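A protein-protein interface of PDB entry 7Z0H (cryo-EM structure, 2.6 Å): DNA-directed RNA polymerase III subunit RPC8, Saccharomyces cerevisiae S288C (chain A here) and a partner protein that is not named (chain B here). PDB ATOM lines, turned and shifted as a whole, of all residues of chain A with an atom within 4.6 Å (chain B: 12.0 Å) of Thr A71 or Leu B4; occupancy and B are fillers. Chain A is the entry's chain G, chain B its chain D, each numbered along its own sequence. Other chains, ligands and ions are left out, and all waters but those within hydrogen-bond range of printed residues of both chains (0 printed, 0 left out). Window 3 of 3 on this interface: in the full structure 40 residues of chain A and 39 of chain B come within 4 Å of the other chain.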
ATOM      1  N   LYS A   6      -1.261 -21.954 -27.386  1.00  0.00           N
ATOM      2  CA  LYS A   6       0.177 -22.078 -27.197  1.00  0.00           C
ATOM      3  C   LYS A   6       0.684 -20.942 -26.318  1.00  0.00           C
ATOM      4  O   LYS A   6       0.374 -19.770 -26.554  1.00  0.00           O
ATOM      5  CB  LYS A   6       0.912 -22.114 -28.540  1.00  0.00           C
ATOM      6  CG  LYS A   6       0.878 -20.830 -29.346  1.00  0.00           C
ATOM      7  CD  LYS A   6       1.557 -21.002 -30.698  1.00  0.00           C
ATOM      8  CE  LYS A   6       2.880 -21.745 -30.576  1.00  0.00           C
ATOM      9  NZ  LYS A   6       3.794 -21.451 -31.716  1.00  0.00           N
ATOM     10  N   ILE A   7       1.437 -21.305 -25.284  1.00  0.00           N
ATOM     11  CA  ILE A   7       1.955 -20.363 -24.304  1.00  0.00           C
ATOM     12  C   ILE A   7       3.457 -20.568 -24.189  1.00  0.00           C
ATOM     13  O   ILE A   7       3.941 -21.705 -24.197  1.00  0.00           O
ATOM     14  CB  ILE A   7       1.274 -20.538 -22.930  1.00  0.00           C
ATOM     15  CG1 ILE A   7      -0.249 -20.555 -23.077  1.00  0.00           C
ATOM     16  CG2 ILE A   7       1.703 -19.442 -21.975  1.00  0.00           C
ATOM     17  CD1 ILE A   7      -0.990 -20.583 -21.757  1.00  0.00           C
ATOM     18  N   ALA A   8       4.195 -19.466 -24.100  1.00  0.00           N
ATOM     19  CA  ALA A   8       5.631 -19.489 -23.866  1.00  0.00           C
ATOM     20  C   ALA A   8       5.891 -19.096 -22.420  1.00  0.00           C
ATOM     21  O   ALA A   8       5.377 -18.075 -21.953  1.00  0.00           O
ATOM     22  CB  ALA A   8       6.360 -18.541 -24.820  1.00  0.00           C
ATOM     23  N   LEU A  51       4.560 -30.432 -25.318  1.00  0.00           N
ATOM     24  CA  LEU A  51       5.628 -29.446 -25.339  1.00  0.00           C
ATOM     25  C   LEU A  51       6.182 -29.305 -26.750  1.00  0.00           C
ATOM     26  O   LEU A  51       6.108 -30.226 -27.567  1.00  0.00           O
ATOM     27  CB  LEU A  51       6.760 -29.830 -24.376  1.00  0.00           C
ATOM     28  CG  LEU A  51       6.360 -30.169 -22.939  1.00  0.00           C
ATOM     29  CD1 LEU A  51       7.521 -30.818 -22.202  1.00  0.00           C
ATOM     30  CD2 LEU A  51       5.885 -28.925 -22.208  1.00  0.00           C
ATOM     31  N   LEU A  52       6.651 -28.099 -27.082  1.00  0.00           N
ATOM     32  CA  LEU A  52       7.094 -27.849 -28.482  1.00  0.00           C
ATOM     33  C   LEU A  52       8.561 -27.411 -28.506  1.00  0.00           C
ATOM     34  O   LEU A  52       9.396 -28.179 -29.010  1.00  0.00           O
ATOM     35  CB  LEU A  52       6.195 -26.770 -29.093  1.00  0.00           C
ATOM     36  CG  LEU A  52       4.773 -26.705 -28.539  1.00  0.00           C
ATOM     37  CD1 LEU A  52       4.174 -25.323 -28.743  1.00  0.00           C
ATOM     38  CD2 LEU A  52       3.893 -27.767 -29.180  1.00  0.00           C
ATOM     39  N   THR A  53       8.847 -26.204 -28.014  1.00  0.00           N
ATOM     40  CA  THR A  53      10.247 -25.704 -27.991  1.00  0.00           C
ATOM     41  C   THR A  53      10.791 -25.796 -26.563  1.00  0.00           C
ATOM     42  O   THR A  53      10.308 -25.039 -25.702  1.00  0.00           O
ATOM     43  CB  THR A  53      10.349 -24.282 -28.555  1.00  0.00           C
ATOM     44  OG1 THR A  53       9.903 -24.313 -29.911  1.00  0.00           O
ATOM     45  CG2 THR A  53      11.752 -23.721 -28.488  1.00  0.00           C
ATOM     46  N   ASN A  69      13.338 -22.082 -20.938  1.00  0.00           N
ATOM     47  CA  ASN A  69      12.358 -21.405 -21.780  1.00  0.00           C
ATOM     48  C   ASN A  69      11.605 -22.470 -22.565  1.00  0.00           C
ATOM     49  O   ASN A  69      12.203 -23.211 -23.351  1.00  0.00           O
ATOM     50  CB  ASN A  69      13.041 -20.412 -22.715  1.00  0.00           C
ATOM     51  CG  ASN A  69      13.407 -19.117 -22.023  1.00  0.00           C
ATOM     52  OD1 ASN A  69      14.530 -18.629 -22.150  1.00  0.00           O
ATOM     53  ND2 ASN A  69      12.458 -18.551 -21.289  1.00  0.00           N
ATOM     54  N   VAL A  70      10.296 -22.559 -22.350  1.00  0.00           N
ATOM     55  CA  VAL A  70       9.483 -23.610 -22.945  1.00  0.00           C
ATOM     56  C   VAL A  70       8.238 -22.995 -23.568  1.00  0.00           C
ATOM     57  O   VAL A  70       7.624 -22.086 -22.999  1.00  0.00           O
ATOM     58  CB  VAL A  70       9.109 -24.696 -21.909  1.00  0.00           C
ATOM     59  CG1 VAL A  70       8.219 -24.131 -20.814  1.00  0.00           C
ATOM     60  CG2 VAL A  70       8.427 -25.869 -22.591  1.00  0.00           C
ATOM     61  N   THR A  71       7.895 -23.465 -24.762  1.00  0.00           N
ATOM     62  CA  THR A  71       6.606 -23.200 -25.379  1.00  0.00           C
ATOM     63  C   THR A  71       5.787 -24.482 -25.331  1.00  0.00           C
ATOM     64  O   THR A  71       6.328 -25.579 -25.496  1.00  0.00           O
ATOM     65  CB  THR A  71       6.757 -22.727 -26.825  1.00  0.00           C
ATOM     66  OG1 THR A  71       7.585 -23.645 -27.544  1.00  0.00           O
ATOM     67  CG2 THR A  71       7.392 -21.350 -26.869  1.00  0.00           C
ATOM     68  N   PHE A  72       4.491 -24.348 -25.079  1.00  0.00           N
ATOM     69  CA  PHE A  72       3.660 -25.525 -24.903  1.00  0.00           C
ATOM     70  C   PHE A  72       2.239 -25.212 -25.336  1.00  0.00           C
ATOM     71  O   PHE A  72       1.812 -24.055 -25.351  1.00  0.00           O
ATOM     72  CB  PHE A  72       3.679 -26.012 -23.449  1.00  0.00           C
ATOM     73  CG  PHE A  72       3.117 -25.021 -22.467  1.00  0.00           C
ATOM     74  CD1 PHE A  72       3.859 -23.924 -22.067  1.00  0.00           C
ATOM     75  CD2 PHE A  72       1.847 -25.190 -21.943  1.00  0.00           C
ATOM     76  CE1 PHE A  72       3.346 -23.012 -21.166  1.00  0.00           C
ATOM     77  CE2 PHE A  72       1.328 -24.281 -21.041  1.00  0.00           C
ATOM     78  CZ  PHE A  72       2.080 -23.191 -20.653  1.00  0.00           C
ATOM     79  N   MET B   1       5.555 -16.595 -19.929  1.00  0.00           N
ATOM     80  CA  MET B   1       4.174 -16.396 -19.503  1.00  0.00           C
ATOM     81  C   MET B   1       3.390 -15.940 -20.724  1.00  0.00           C
ATOM     82  O   MET B   1       2.363 -16.524 -21.060  1.00  0.00           O
ATOM     83  CB  MET B   1       4.088 -15.353 -18.385  1.00  0.00           C
ATOM     84  CG  MET B   1       2.683 -14.862 -17.961  1.00  0.00           C
ATOM     85  SD  MET B   1       1.543 -16.069 -17.224  1.00  0.00           S
ATOM     86  CE  MET B   1       0.584 -16.665 -18.610  1.00  0.00           C
ATOM     87  N   LYS B   2       3.917 -14.909 -21.394  1.00  0.00           N
ATOM     88  CA  LYS B   2       3.238 -14.260 -22.513  1.00  0.00           C
ATOM     89  C   LYS B   2       2.657 -15.285 -23.473  1.00  0.00           C
ATOM     90  O   LYS B   2       3.376 -16.143 -23.995  1.00  0.00           O
ATOM     91  CB  LYS B   2       4.209 -13.335 -23.256  1.00  0.00           C
ATOM     92  CG  LYS B   2       3.535 -12.211 -24.039  1.00  0.00           C
ATOM     93  CD  LYS B   2       3.632 -10.886 -23.301  1.00  0.00           C
ATOM     94  CE  LYS B   2       5.075 -10.556 -22.951  1.00  0.00           C
ATOM     95  NZ  LYS B   2       5.202  -9.195 -22.362  1.00  0.00           N
ATOM     96  N   VAL B   3       1.349 -15.195 -23.692  1.00  0.00           N
ATOM     97  CA  VAL B   3       0.636 -16.162 -24.519  1.00  0.00           C
ATOM     98  C   VAL B   3       0.938 -15.859 -25.979  1.00  0.00           C
ATOM     99  O   VAL B   3       0.753 -14.730 -26.442  1.00  0.00           O
ATOM    100  CB  VAL B   3      -0.873 -16.121 -24.242  1.00  0.00           C
ATOM    101  CG1 VAL B   3      -1.651 -16.656 -25.433  1.00  0.00           C
ATOM    102  CG2 VAL B   3      -1.204 -16.914 -22.986  1.00  0.00           C
ATOM    103  N   LEU B   4       1.417 -16.871 -26.706  1.00  0.00           N
ATOM    104  CA  LEU B   4       1.816 -16.659 -28.092  1.00  0.00           C
ATOM    105  C   LEU B   4       0.612 -16.347 -28.974  1.00  0.00           C
ATOM    106  O   LEU B   4       0.646 -15.404 -29.772  1.00  0.00           O
ATOM    107  CB  LEU B   4       2.577 -17.879 -28.607  1.00  0.00           C
ATOM    108  CG  LEU B   4       3.997 -18.028 -28.055  1.00  0.00           C
ATOM    109  CD1 LEU B   4       4.606 -19.360 -28.458  1.00  0.00           C
ATOM    110  CD2 LEU B   4       4.870 -16.872 -28.520  1.00  0.00           C
ATOM    111  N   GLU B   5      -0.465 -17.124 -28.843  1.00  0.00           N
ATOM    112  CA  GLU B   5      -1.694 -16.835 -29.574  1.00  0.00           C
ATOM    113  C   GLU B   5      -2.850 -17.580 -28.923  1.00  0.00           C
ATOM    114  O   GLU B   5      -2.733 -18.769 -28.611  1.00  0.00           O
ATOM    115  CB  GLU B   5      -1.557 -17.198 -31.060  1.00  0.00           C
ATOM    116  CG  GLU B   5      -1.114 -18.613 -31.346  1.00  0.00           C
ATOM    117  CD  GLU B   5      -2.224 -19.455 -31.924  1.00  0.00           C
ATOM    118  OE1 GLU B   5      -3.171 -18.876 -32.492  1.00  0.00           O
ATOM    119  OE2 GLU B   5      -2.144 -20.693 -31.823  1.00  0.00           O
ATOM    120  N   GLU B   6      -3.960 -16.867 -28.722  1.00  0.00           N
ATOM    121  CA  GLU B   6      -5.056 -17.378 -27.904  1.00  0.00           C
ATOM    122  C   GLU B   6      -5.780 -18.539 -28.577  1.00  0.00           C
ATOM    123  O   GLU B   6      -6.210 -19.481 -27.902  1.00  0.00           O
ATOM    124  CB  GLU B   6      -6.034 -16.245 -27.592  1.00  0.00           C
ATOM    125  CG  GLU B   6      -7.149 -16.610 -26.628  1.00  0.00           C
ATOM    126  CD  GLU B   6      -8.284 -15.602 -26.645  1.00  0.00           C
ATOM    127  OE1 GLU B   6      -8.439 -14.896 -27.664  1.00  0.00           O
ATOM    128  OE2 GLU B   6      -9.021 -15.514 -25.640  1.00  0.00           O
ATOM    129  N   ARG B   7      -5.927 -18.492 -29.897  1.00  0.00           N
ATOM    130  CA  ARG B   7      -6.797 -19.416 -30.624  1.00  0.00           C
ATOM    131  C   ARG B   7      -5.944 -20.403 -31.421  1.00  0.00           C
ATOM    132  O   ARG B   7      -5.600 -20.156 -32.578  1.00  0.00           O
ATOM    133  CB  ARG B   7      -7.750 -18.643 -31.530  1.00  0.00           C
ATOM    134  CG  ARG B   7      -9.035 -19.379 -31.867  1.00  0.00           C
ATOM    135  CD  ARG B   7      -9.995 -18.485 -32.633  1.00  0.00           C
ATOM    136  NE  ARG B   7     -10.433 -17.345 -31.836  1.00  0.00           N
ATOM    137  CZ  ARG B   7      -9.960 -16.112 -31.965  1.00  0.00           C
ATOM    138  NH1 ARG B   7      -9.028 -15.819 -32.857  1.00  0.00           N
ATOM    139  NH2 ARG B   7     -10.431 -15.151 -31.177  1.00  0.00           N
ATOM    140  N   ASN B   8      -5.624 -21.533 -30.796  1.00  0.00           N
ATOM    141  CA  ASN B   8      -4.936 -22.632 -31.457  1.00  0.00           C
ATOM    142  C   ASN B   8      -5.938 -23.567 -32.127  1.00  0.00           C
ATOM    143  O   ASN B   8      -7.114 -23.240 -32.306  1.00  0.00           O
ATOM    144  CB  ASN B   8      -4.067 -23.407 -30.472  1.00  0.00           C
ATOM    145  CG  ASN B   8      -2.602 -23.376 -30.839  1.00  0.00           C
ATOM    146  OD1 ASN B   8      -2.245 -23.480 -32.012  1.00  0.00           O
ATOM    147  ND2 ASN B   8      -1.745 -23.258 -29.842  1.00  0.00           N
ATOM    148  N   ALA B   9      -5.458 -24.744 -32.519  1.00  0.00           N
ATOM    149  CA  ALA B   9      -6.320 -25.758 -33.106  1.00  0.00           C
ATOM    150  C   ALA B   9      -7.403 -26.175 -32.118  1.00  0.00           C
ATOM    151  O   ALA B   9      -7.189 -26.222 -30.904  1.00  0.00           O
ATOM    152  CB  ALA B   9      -5.496 -26.975 -33.529  1.00  0.00           C
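The backbone NH of Leu B4 is in hydrogen-bond range of the backbone carbonyl oxygen of Lys A6. ND2 of Asn B8 lies close to N of Lys A6, 2.8 Å away. The backbone carbonyl oxygen of Ala A8 sits at hydrogen-bond distance from the backbone NH of Met B1. The backbone NH of Ala A8 lies within hydrogen-bond range of the backbone carbonyl oxygen of Lys B2, 3.4 Å away.
The backbone NH of Leu A52 lies within hydrogen-bond range of the backbone carbonyl oxygen of Thr A71. N of Ile A7 lies within hydrogen-bond range of O of Phe A72. OG1 of Thr A71 sits at hydrogen-bond distance from N of Thr A53 (2.9 Å). OE1 of Glu B5 sits close to O of Arg B7, at 2.7 Å. The side-chain carboxylate (OE2) of Glu B5 lies close to the side-chain amide oxygen (OD1) of Asn B8 (2.8 Å).
Among the printed residues, merely in contact across the chains: Lys A6 with Val B3, Lys A6 with Glu B5, Ile A7 with Met B1, Ile A7 with Val B3 and Thr A71 with Leu B4.
Lys A6 touches just these residues of chain B: Val B3, Leu B4, Glu B5 and Asn B8. Of chain B, only Met B1 and Val B3 come within 4 Å of Ile A7. Ala A8 touches just these residues of chain B: Met B1 and Lys B2. Leu A52 touches none of the printed residues of chain B. Thr A53 touches none of the printed residues of chain B. Thr A71 touches one residue of chain B. Of the printed residues of chain A, Met B1 touches Ile A7 (3.1 Å) and Ala A8 (2.5 Å). Of chain A, only Lys A6 (3.1 Å) and Thr A71 (3.8 Å) come within 4 Å of Leu B4. Of the printed residues of chain A, Glu B5 touches Lys A6 (3.6 Å). Printed residues of chain A within 4 Å of Asn B8: Lys A6. Ala B9 touches none of the printed residues of chain A. The nearest residue of chain A that does not touch Leu B4 is Ala A8 (4.04 Å). The nearest printed residue of chain A that does not touch Glu B5 is Ile A7 (5.8 Å).
Hydrophobic or aromatic side chains of chain B that line the printed part of chain A: Val B3 and Leu B4. Among the printed residues, no Asp or Glu carboxylate lies within 4 Å of a Lys or Arg side-chain nitrogen of the other chain.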
